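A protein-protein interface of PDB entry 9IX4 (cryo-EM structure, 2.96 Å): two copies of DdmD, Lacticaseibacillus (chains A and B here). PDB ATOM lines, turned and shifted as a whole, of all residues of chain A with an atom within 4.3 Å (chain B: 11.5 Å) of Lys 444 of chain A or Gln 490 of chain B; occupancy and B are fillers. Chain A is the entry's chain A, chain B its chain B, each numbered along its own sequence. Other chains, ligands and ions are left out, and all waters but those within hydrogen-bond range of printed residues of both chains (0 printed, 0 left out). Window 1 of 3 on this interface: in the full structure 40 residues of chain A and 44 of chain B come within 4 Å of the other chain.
The guanidinium group (NH1) of Arg 242 of chain A is in salt-bridge range of the side-chain carboxylate (OD2) of Asp 488 of chain B, at 3.0 Å. The backbone carbonyl oxygen (O) of Pro 489 of chain B sits at hydrogen-bond distance from the side-chain hydroxyl (OG) of Ser 435 of chain A (3.1 Å). N of Ser 435 of chain A lies within hydrogen-bond range of O of Gln 490 of chain B, 3.1 Å away. The side-chain amino group (NZ) of Lys 444 of chain A lies within hydrogen-bond range of the side-chain amide oxygen (OE1) of Gln 490 of chain B, at 2.8 Å. O of Phe 434 of chain A lies close to O of Gln 490 of chain B, at 3.2 Å.
The backbone carbonyl oxygen of Asp 431 of chain A lies within hydrogen-bond range of the side-chain hydroxyl of Ser 435 of chain A (2.5 Å). The backbone carbonyl oxygen (O) of Asp 492 of chain B is in hydrogen-bond range of the side-chain amino group (NZ) of Lys 338 of chain B, 3.1 Å away. The side-chain carboxylate (OD2) of Asp 488 of chain B lies within hydrogen-bond range of the backbone NH (N) of Gln 490 of chain B (3.1 Å).
Gln 490 of chain B touches Arg 242 of chain A. O of Pro 489 of chain B touches O of Asp 431 of chain A (3.98 Å). OD1 of Asp 431 of chain A touches CG of Gln 490 of chain B, at 3.5 Å. OG of Ser 435 of chain A touches N of Asp 492 of chain B, at 3.5 Å. Ser 435 of chain A touches Leu 493 of chain B.
Of the printed residues of chain B, Arg 242 of chain A touches Asp 488 and Gln 490. Printed residues of chain B within 4 Å of Asp 431 of chain A: Pro 489 and Gln 490. Phe 434 of chain A touches one residue of chain B. Of the printed residues of chain B, Ser 435 of chain A touches Pro 489, Gln 490, Asp 492 and Leu 493. Printed residues of chain B within 4 Å of Lys 444 of chain A: Gln 490. No residue of chain B comes within 4 Å of Ala 447 of chain A. No residue of chain B comes within 4 Å of Lys 448 of chain A. Of the printed residues of chain A, Asp 488 of chain B touches Arg 242 (3.0 Å). Of chain A, only Arg 242, Asp 431, Phe 434, Ser 435 and Lys 444 come within 4 Å of Gln 490 of chain B. Of the printed residues of chain A, Asp 492 of chain B touches Ser 435. Printed residues of chain A within 4 Å of Leu 493 of chain B: Ser 435 (3.6 Å). The nearest residue of chain B that does not touch Lys 444 of chain A is Asp 488 of chain B (5.7 Å).
Printed residues of chain B that touch a printed residue of chain A: Asp 488, Pro 489, Gln 490, Asp 492 and Leu 493. Printed residues of chain A that touch a printed residue of chain B: Arg 242, Asp 431, Phe 434, Ser 435 and Lys 444. Among the printed residues, 10 pairs touch across the chains. Among the printed residues, Asp or Glu carboxylates within 4 Å of a Lys or Arg side-chain nitrogen of the other chain: Arg 242 of chain A with Asp 488 of chain B.
Positions printed for both chains: 442, 443, 444, 445 and 446. Of the 10 pairs that touch across the chains among the printed residues, none has its exchanged pair printed and touching as well.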
ATOM      1  N   ARG A 242       7.590  -1.533  19.503  1.00  0.00           N
ATOM      2  CA  ARG A 242       8.336  -0.619  18.649  1.00  0.00           C
ATOM      3  C   ARG A 242       7.400   0.456  18.114  1.00  0.00           C
ATOM      4  O   ARG A 242       6.392   0.144  17.473  1.00  0.00           O
ATOM      5  CB  ARG A 242       8.985  -1.388  17.502  1.00  0.00           C
ATOM      6  CG  ARG A 242       9.664  -0.517  16.467  1.00  0.00           C
ATOM      7  CD  ARG A 242      10.516  -1.352  15.536  1.00  0.00           C
ATOM      8  NE  ARG A 242      11.483  -2.164  16.263  1.00  0.00           N
ATOM      9  CZ  ARG A 242      12.267  -3.073  15.699  1.00  0.00           C
ATOM     10  NH1 ARG A 242      12.218  -3.318  14.400  1.00  0.00           N
ATOM     11  NH2 ARG A 242      13.119  -3.755  16.458  1.00  0.00           N
ATOM     12  N   ASP A 431      10.831   0.734   6.585  1.00  0.00           N
ATOM     13  CA  ASP A 431      11.206  -0.662   6.762  1.00  0.00           C
ATOM     14  C   ASP A 431      11.901  -1.205   5.525  1.00  0.00           C
ATOM     15  O   ASP A 431      12.898  -1.923   5.632  1.00  0.00           O
ATOM     16  CB  ASP A 431       9.977  -1.503   7.092  1.00  0.00           C
ATOM     17  CG  ASP A 431       9.453  -1.243   8.484  1.00  0.00           C
ATOM     18  OD1 ASP A 431      10.214  -0.709   9.315  1.00  0.00           O
ATOM     19  OD2 ASP A 431       8.281  -1.576   8.750  1.00  0.00           O
ATOM     20  N   PHE A 434      15.455   0.299   5.340  1.00  0.00           N
ATOM     21  CA  PHE A 434      16.338  -0.315   6.322  1.00  0.00           C
ATOM     22  C   PHE A 434      16.680  -1.744   5.930  1.00  0.00           C
ATOM     23  O   PHE A 434      17.816  -2.187   6.111  1.00  0.00           O
ATOM     24  CB  PHE A 434      15.696  -0.275   7.705  1.00  0.00           C
ATOM     25  CG  PHE A 434      15.863   1.036   8.405  1.00  0.00           C
ATOM     26  CD1 PHE A 434      16.618   2.042   7.840  1.00  0.00           C
ATOM     27  CD2 PHE A 434      15.265   1.265   9.626  1.00  0.00           C
ATOM     28  CE1 PHE A 434      16.773   3.248   8.478  1.00  0.00           C
ATOM     29  CE2 PHE A 434      15.419   2.471  10.268  1.00  0.00           C
ATOM     30  CZ  PHE A 434      16.174   3.463   9.692  1.00  0.00           C
ATOM     31  N   SER A 435      15.709  -2.480   5.388  1.00  0.00           N
ATOM     32  CA  SER A 435      15.970  -3.843   4.950  1.00  0.00           C
ATOM     33  C   SER A 435      16.993  -3.873   3.828  1.00  0.00           C
ATOM     34  O   SER A 435      17.906  -4.704   3.835  1.00  0.00           O
ATOM     35  CB  SER A 435      14.670  -4.503   4.502  1.00  0.00           C
ATOM     36  OG  SER A 435      13.641  -4.272   5.442  1.00  0.00           O
ATOM     37  N   LEU A 442      25.298  -3.012   5.817  1.00  0.00           N
ATOM     38  CA  LEU A 442      25.496  -1.727   6.465  1.00  0.00           C
ATOM     39  C   LEU A 442      24.969  -1.787   7.890  1.00  0.00           C
ATOM     40  O   LEU A 442      23.955  -2.434   8.161  1.00  0.00           O
ATOM     41  CB  LEU A 442      24.794  -0.610   5.695  1.00  0.00           C
ATOM     42  CG  LEU A 442      25.528  -0.076   4.470  1.00  0.00           C
ATOM     43  CD1 LEU A 442      24.538   0.404   3.442  1.00  0.00           C
ATOM     44  CD2 LEU A 442      26.449   1.046   4.867  1.00  0.00           C
ATOM     45  N   SER A 443      25.663  -1.112   8.795  1.00  0.00           N
ATOM     46  CA  SER A 443      25.247  -1.090  10.184  1.00  0.00           C
ATOM     47  C   SER A 443      23.932  -0.333  10.331  1.00  0.00           C
ATOM     48  O   SER A 443      23.496   0.388   9.434  1.00  0.00           O
ATOM     49  CB  SER A 443      26.325  -0.447  11.051  1.00  0.00           C
ATOM     50  OG  SER A 443      25.880  -0.307  12.385  1.00  0.00           O
ATOM     51  N   LYS A 444      23.293  -0.514  11.486  1.00  0.00           N
ATOM     52  CA  LYS A 444      22.034   0.177  11.741  1.00  0.00           C
ATOM     53  C   LYS A 444      22.231   1.687  11.753  1.00  0.00           C
ATOM     54  O   LYS A 444      21.395   2.430  11.230  1.00  0.00           O
ATOM     55  CB  LYS A 444      21.432  -0.301  13.059  1.00  0.00           C
ATOM     56  CG  LYS A 444      20.026   0.199  13.313  1.00  0.00           C
ATOM     57  CD  LYS A 444      19.076  -0.278  12.236  1.00  0.00           C
ATOM     58  CE  LYS A 444      17.639   0.057  12.581  1.00  0.00           C
ATOM     59  NZ  LYS A 444      17.107  -0.834  13.645  1.00  0.00           N
ATOM     60  N   SER A 445      23.328   2.157  12.347  1.00  0.00           N
ATOM     61  CA  SER A 445      23.615   3.587  12.347  1.00  0.00           C
ATOM     62  C   SER A 445      23.879   4.102  10.940  1.00  0.00           C
ATOM     63  O   SER A 445      23.408   5.185  10.567  1.00  0.00           O
ATOM     64  CB  SER A 445      24.812   3.872  13.247  1.00  0.00           C
ATOM     65  OG  SER A 445      24.563   3.432  14.567  1.00  0.00           O
ATOM     66  N   GLN A 446      24.644   3.349  10.151  1.00  0.00           N
ATOM     67  CA  GLN A 446      24.912   3.755   8.779  1.00  0.00           C
ATOM     68  C   GLN A 446      23.632   3.781   7.962  1.00  0.00           C
ATOM     69  O   GLN A 446      23.409   4.704   7.173  1.00  0.00           O
ATOM     70  CB  GLN A 446      25.936   2.815   8.153  1.00  0.00           C
ATOM     71  CG  GLN A 446      27.265   2.809   8.874  1.00  0.00           C
ATOM     72  CD  GLN A 446      28.301   1.966   8.175  1.00  0.00           C
ATOM     73  OE1 GLN A 446      28.048   0.819   7.821  1.00  0.00           O
ATOM     74  NE2 GLN A 446      29.482   2.529   7.979  1.00  0.00           N
ATOM     75  N   ALA A 447      22.773   2.780   8.147  1.00  0.00           N
ATOM     76  CA  ALA A 447      21.487   2.779   7.467  1.00  0.00           C
ATOM     77  C   ALA A 447      20.654   3.982   7.877  1.00  0.00           C
ATOM     78  O   ALA A 447      20.001   4.609   7.039  1.00  0.00           O
ATOM     79  CB  ALA A 447      20.738   1.486   7.769  1.00  0.00           C
ATOM     80  N   LYS A 448      20.668   4.318   9.164  1.00  0.00           N
ATOM     81  CA  LYS A 448      19.889   5.449   9.648  1.00  0.00           C
ATOM     82  C   LYS A 448      20.357   6.748   9.007  1.00  0.00           C
ATOM     83  O   LYS A 448      19.544   7.545   8.523  1.00  0.00           O
ATOM     84  CB  LYS A 448      19.992   5.520  11.169  1.00  0.00           C
ATOM     85  CG  LYS A 448      19.067   6.511  11.820  1.00  0.00           C
ATOM     86  CD  LYS A 448      19.317   6.547  13.312  1.00  0.00           C
ATOM     87  CE  LYS A 448      18.844   5.264  13.970  1.00  0.00           C
ATOM     88  NZ  LYS A 448      18.992   5.317  15.447  1.00  0.00           N
ATOM     89  N   ASP B 283      25.863 -10.883  14.917  1.00  0.00           N
ATOM     90  CA  ASP B 283      25.495 -11.752  13.809  1.00  0.00           C
ATOM     91  C   ASP B 283      26.732 -12.482  13.317  1.00  0.00           C
ATOM     92  O   ASP B 283      27.700 -11.850  12.888  1.00  0.00           O
ATOM     93  CB  ASP B 283      24.868 -10.931  12.688  1.00  0.00           C
ATOM     94  CG  ASP B 283      24.427 -11.781  11.514  1.00  0.00           C
ATOM     95  OD1 ASP B 283      24.113 -12.969  11.719  1.00  0.00           O
ATOM     96  OD2 ASP B 283      24.389 -11.257  10.383  1.00  0.00           O
ATOM     97  N   SER B 286      27.754 -11.940   9.348  1.00  0.00           N
ATOM     98  CA  SER B 286      28.315 -10.628   9.059  1.00  0.00           C
ATOM     99  C   SER B 286      29.651 -10.438   9.758  1.00  0.00           C
ATOM    100  O   SER B 286      30.568  -9.832   9.200  1.00  0.00           O
ATOM    101  CB  SER B 286      27.335  -9.535   9.472  1.00  0.00           C
ATOM    102  OG  SER B 286      27.300  -9.409  10.879  1.00  0.00           O
ATOM    103  N   ASP B 290      32.968  -9.650   7.633  1.00  0.00           N
ATOM    104  CA  ASP B 290      33.706  -8.416   7.859  1.00  0.00           C
ATOM    105  C   ASP B 290      35.145  -8.691   8.267  1.00  0.00           C
ATOM    106  O   ASP B 290      36.065  -8.004   7.811  1.00  0.00           O
ATOM    107  CB  ASP B 290      32.999  -7.574   8.917  1.00  0.00           C
ATOM    108  CG  ASP B 290      31.689  -7.002   8.426  1.00  0.00           C
ATOM    109  OD1 ASP B 290      31.549  -6.803   7.202  1.00  0.00           O
ATOM    110  OD2 ASP B 290      30.802  -6.743   9.262  1.00  0.00           O
ATOM    111  N   LEU B 336      22.880 -14.211   1.626  1.00  0.00           N
ATOM    112  CA  LEU B 336      22.068 -13.970   2.807  1.00  0.00           C
ATOM    113  C   LEU B 336      21.383 -15.256   3.243  1.00  0.00           C
ATOM    114  O   LEU B 336      20.827 -15.981   2.416  1.00  0.00           O
ATOM    115  CB  LEU B 336      21.025 -12.888   2.532  1.00  0.00           C
ATOM    116  CG  LEU B 336      21.563 -11.517   2.130  1.00  0.00           C
ATOM    117  CD1 LEU B 336      20.432 -10.535   1.947  1.00  0.00           C
ATOM    118  CD2 LEU B 336      22.544 -11.006   3.159  1.00  0.00           C
ATOM    119  N   LYS B 338      18.292 -16.717   4.866  1.00  0.00           N
ATOM    120  CA  LYS B 338      16.916 -16.343   5.162  1.00  0.00           C
ATOM    121  C   LYS B 338      16.194 -17.543   5.749  1.00  0.00           C
ATOM    122  O   LYS B 338      16.123 -18.601   5.118  1.00  0.00           O
ATOM    123  CB  LYS B 338      16.196 -15.836   3.916  1.00  0.00           C
ATOM    124  CG  LYS B 338      14.825 -15.274   4.212  1.00  0.00           C
ATOM    125  CD  LYS B 338      14.892 -14.261   5.328  1.00  0.00           C
ATOM    126  CE  LYS B 338      13.519 -13.959   5.876  1.00  0.00           C
ATOM    127  NZ  LYS B 338      12.616 -13.465   4.816  1.00  0.00           N
ATOM    128  N   LEU B 442      36.035  -3.129  11.231  1.00  0.00           N
ATOM    129  CA  LEU B 442      34.998  -3.740  12.042  1.00  0.00           C
ATOM    130  C   LEU B 442      34.301  -2.696  12.901  1.00  0.00           C
ATOM    131  O   LEU B 442      34.875  -1.663  13.250  1.00  0.00           O
ATOM    132  CB  LEU B 442      35.603  -4.820  12.931  1.00  0.00           C
ATOM    133  CG  LEU B 442      36.176  -6.006  12.172  1.00  0.00           C
ATOM    134  CD1 LEU B 442      37.079  -6.792  13.064  1.00  0.00           C
ATOM    135  CD2 LEU B 442      35.049  -6.875  11.707  1.00  0.00           C
ATOM    136  N   SER B 443      33.051  -2.979  13.247  1.00  0.00           N
ATOM    137  CA  SER B 443      32.302  -2.096  14.122  1.00  0.00           C
ATOM    138  C   SER B 443      32.812  -2.217  15.555  1.00  0.00           C
ATOM    139  O   SER B 443      33.621  -3.085  15.886  1.00  0.00           O
ATOM    140  CB  SER B 443      30.813  -2.420  14.062  1.00  0.00           C
ATOM    141  OG  SER B 443      30.084  -1.595  14.947  1.00  0.00           O
ATOM    142  N   LYS B 444      32.341  -1.312  16.411  1.00  0.00           N
ATOM    143  CA  LYS B 444      32.728  -1.367  17.815  1.00  0.00           C
ATOM    144  C   LYS B 444      32.182  -2.618  18.493  1.00  0.00           C
ATOM    145  O   LYS B 444      32.884  -3.258  19.283  1.00  0.00           O
ATOM    146  CB  LYS B 444      32.258  -0.110  18.539  1.00  0.00           C
ATOM    147  CG  LYS B 444      32.830   0.030  19.930  1.00  0.00           C
ATOM    148  CD  LYS B 444      34.337  -0.129  19.920  1.00  0.00           C
ATOM    149  CE  LYS B 444      34.905  -0.105  21.328  1.00  0.00           C
ATOM    150  NZ  LYS B 444      35.004   1.275  21.878  1.00  0.00           N
ATOM    151  N   SER B 445      30.932  -2.978  18.203  1.00  0.00           N
ATOM    152  CA  SER B 445      30.364  -4.196  18.771  1.00  0.00           C
ATOM    153  C   SER B 445      31.080  -5.435  18.251  1.00  0.00           C
ATOM    154  O   SER B 445      31.328  -6.383  19.006  1.00  0.00           O
ATOM    155  CB  SER B 445      28.874  -4.266  18.457  1.00  0.00           C
ATOM    156  OG  SER B 445      28.183  -3.212  19.098  1.00  0.00           O
ATOM    157  N   GLN B 446      31.410  -5.448  16.962  1.00  0.00           N
ATOM    158  CA  GLN B 446      32.154  -6.567  16.403  1.00  0.00           C
ATOM    159  C   GLN B 446      33.543  -6.655  17.016  1.00  0.00           C
ATOM    160  O   GLN B 446      34.046  -7.752  17.284  1.00  0.00           O
ATOM    161  CB  GLN B 446      32.228  -6.425  14.886  1.00  0.00           C
ATOM    162  CG  GLN B 446      30.864  -6.394  14.233  1.00  0.00           C
ATOM    163  CD  GLN B 446      30.935  -6.296  12.732  1.00  0.00           C
ATOM    164  OE1 GLN B 446      31.719  -5.528  12.188  1.00  0.00           O
ATOM    165  NE2 GLN B 446      30.104  -7.070  12.051  1.00  0.00           N
ATOM    166  N   THR B 486      17.074 -14.731  14.531  1.00  0.00           N
ATOM    167  CA  THR B 486      16.161 -13.614  14.716  1.00  0.00           C
ATOM    168  C   THR B 486      15.737 -13.068  13.363  1.00  0.00           C
ATOM    169  O   THR B 486      16.578 -12.845  12.488  1.00  0.00           O
ATOM    170  CB  THR B 486      16.816 -12.512  15.550  1.00  0.00           C
ATOM    171  OG1 THR B 486      16.939 -12.953  16.905  1.00  0.00           O
ATOM    172  CG2 THR B 486      15.987 -11.247  15.515  1.00  0.00           C
ATOM    173  N   ASN B 487      14.433 -12.864  13.198  1.00  0.00           N
ATOM    174  CA  ASN B 487      13.858 -12.229  12.023  1.00  0.00           C
ATOM    175  C   ASN B 487      13.222 -10.910  12.436  1.00  0.00           C
ATOM    176  O   ASN B 487      12.440 -10.868  13.390  1.00  0.00           O
ATOM    177  CB  ASN B 487      12.810 -13.129  11.368  1.00  0.00           C
ATOM    178  CG  ASN B 487      13.369 -13.941  10.227  1.00  0.00           C
ATOM    179  OD1 ASN B 487      14.478 -13.698   9.761  1.00  0.00           O
ATOM    180  ND2 ASN B 487      12.599 -14.911   9.764  1.00  0.00           N
ATOM    181  N   ASP B 488      13.554  -9.841  11.720  1.00  0.00           N
ATOM    182  CA  ASP B 488      13.001  -8.530  12.007  1.00  0.00           C
ATOM    183  C   ASP B 488      12.535  -7.879  10.714  1.00  0.00           C
ATOM    184  O   ASP B 488      13.170  -8.050   9.669  1.00  0.00           O
ATOM    185  CB  ASP B 488      14.044  -7.639  12.694  1.00  0.00           C
ATOM    186  CG  ASP B 488      13.447  -6.373  13.262  1.00  0.00           C
ATOM    187  OD1 ASP B 488      12.692  -6.462  14.249  1.00  0.00           O
ATOM    188  OD2 ASP B 488      13.735  -5.286  12.723  1.00  0.00           O
ATOM    189  N   PRO B 489      11.430  -7.134  10.748  1.00  0.00           N
ATOM    190  CA  PRO B 489      10.966  -6.465   9.526  1.00  0.00           C
ATOM    191  C   PRO B 489      11.930  -5.423   8.989  1.00  0.00           C
ATOM    192  O   PRO B 489      11.829  -5.076   7.807  1.00  0.00           O
ATOM    193  CB  PRO B 489       9.637  -5.832   9.953  1.00  0.00           C
ATOM    194  CG  PRO B 489       9.701  -5.768  11.432  1.00  0.00           C
ATOM    195  CD  PRO B 489      10.475  -6.968  11.851  1.00  0.00           C
ATOM    196  N   GLN B 490      12.851  -4.907   9.799  1.00  0.00           N
ATOM    197  CA  GLN B 490      13.796  -3.910   9.317  1.00  0.00           C
ATOM    198  C   GLN B 490      15.051  -4.512   8.702  1.00  0.00           C
ATOM    199  O   GLN B 490      15.879  -3.765   8.174  1.00  0.00           O
ATOM    200  CB  GLN B 490      14.183  -2.953  10.440  1.00  0.00           C
ATOM    201  CG  GLN B 490      13.066  -2.013  10.821  1.00  0.00           C
ATOM    202  CD  GLN B 490      13.471  -1.044  11.899  1.00  0.00           C
ATOM    203  OE1 GLN B 490      14.572  -1.126  12.440  1.00  0.00           O
ATOM    204  NE2 GLN B 490      12.587  -0.110  12.215  1.00  0.00           N
ATOM    205  N   HIS B 491      15.222  -5.826   8.772  1.00  0.00           N
ATOM    206  CA  HIS B 491      16.193  -6.556   7.966  1.00  0.00           C
ATOM    207  C   HIS B 491      15.510  -7.765   7.354  1.00  0.00           C
ATOM    208  O   HIS B 491      15.943  -8.911   7.479  1.00  0.00           O
ATOM    209  CB  HIS B 491      17.449  -6.921   8.758  1.00  0.00           C
ATOM    210  CG  HIS B 491      17.209  -7.809   9.938  1.00  0.00           C
ATOM    211  ND1 HIS B 491      16.856  -9.134   9.815  1.00  0.00           N
ATOM    212  CD2 HIS B 491      17.311  -7.568  11.264  1.00  0.00           C
ATOM    213  CE1 HIS B 491      16.732  -9.666  11.016  1.00  0.00           C
ATOM    214  NE2 HIS B 491      17.003  -8.736  11.914  1.00  0.00           N
ATOM    215  N   ASP B 492      14.396  -7.483   6.678  1.00  0.00           N
ATOM    216  CA  ASP B 492      13.475  -8.500   6.191  1.00  0.00           C
ATOM    217  C   ASP B 492      14.127  -9.485   5.234  1.00  0.00           C
ATOM    218  O   ASP B 492      13.601 -10.585   5.045  1.00  0.00           O
ATOM    219  CB  ASP B 492      12.295  -7.810   5.507  1.00  0.00           C
ATOM    220  CG  ASP B 492      11.214  -8.773   5.091  1.00  0.00           C
ATOM    221  OD1 ASP B 492      10.383  -9.137   5.947  1.00  0.00           O
ATOM    222  OD2 ASP B 492      11.189  -9.167   3.908  1.00  0.00           O
ATOM    223  N   LEU B 493      15.249  -9.123   4.625  1.00  0.00           N
ATOM    224  CA  LEU B 493      15.856  -9.958   3.601  1.00  0.00           C
ATOM    225  C   LEU B 493      16.765 -11.049   4.145  1.00  0.00           C
ATOM    226  O   LEU B 493      17.122 -11.954   3.387  1.00  0.00           O
ATOM    227  CB  LEU B 493      16.637  -9.081   2.632  1.00  0.00           C
ATOM    228  CG  LEU B 493      15.730  -8.157   1.830  1.00  0.00           C
ATOM    229  CD1 LEU B 493      16.519  -6.983   1.352  1.00  0.00           C
ATOM    230  CD2 LEU B 493      15.155  -8.910   0.659  1.00  0.00           C
ATOM    231  N   GLN B 494      17.156 -11.004   5.416  1.00  0.00           N
ATOM    232  CA  GLN B 494      18.002 -12.063   5.939  1.00  0.00           C
ATOM    233  C   GLN B 494      17.656 -12.327   7.393  1.00  0.00           C
ATOM    234  O   GLN B 494      16.980 -11.533   8.048  1.00  0.00           O
ATOM    235  CB  GLN B 494      19.492 -11.737   5.830  1.00  0.00           C
ATOM    236  CG  GLN B 494      20.033 -10.816   6.902  1.00  0.00           C
ATOM    237  CD  GLN B 494      20.006  -9.367   6.511  1.00  0.00           C
ATOM    238  OE1 GLN B 494      19.280  -8.967   5.609  1.00  0.00           O
ATOM    239  NE2 GLN B 494      20.824  -8.568   7.176  1.00  0.00           N
ATOM    240  N   THR B 495      18.129 -13.466   7.884  1.00  0.00           N
ATOM    241  CA  THR B 495      17.938 -13.885   9.264  1.00  0.00           C
ATOM    242  C   THR B 495      19.245 -13.718  10.018  1.00  0.00           C
ATOM    243  O   THR B 495      20.292 -14.187   9.563  1.00  0.00           O
ATOM    244  CB  THR B 495      17.477 -15.339   9.332  1.00  0.00           C
ATOM    245  OG1 THR B 495      16.157 -15.441   8.792  1.00  0.00           O
ATOM    246  CG2 THR B 495      17.472 -15.828  10.758  1.00  0.00           C
ATOM    247  N   LYS B 496      19.190 -13.051  11.164  1.00  0.00           N
ATOM    248  CA  LYS B 496      20.395 -12.812  11.940  1.00  0.00           C
ATOM    249  C   LYS B 496      20.671 -13.994  12.854  1.00  0.00           C
ATOM    250  O   LYS B 496      19.781 -14.458  13.567  1.00  0.00           O
ATOM    251  CB  LYS B 496      20.260 -11.531  12.755  1.00  0.00           C
ATOM    252  CG  LYS B 496      20.760 -10.307  12.029  1.00  0.00           C
ATOM    253  CD  LYS B 496      20.725  -9.090  12.918  1.00  0.00           C
ATOM    254  CE  LYS B 496      21.334  -7.894  12.219  1.00  0.00           C
ATOM    255  NZ  LYS B 496      21.371  -6.705  13.111  1.00  0.00           N
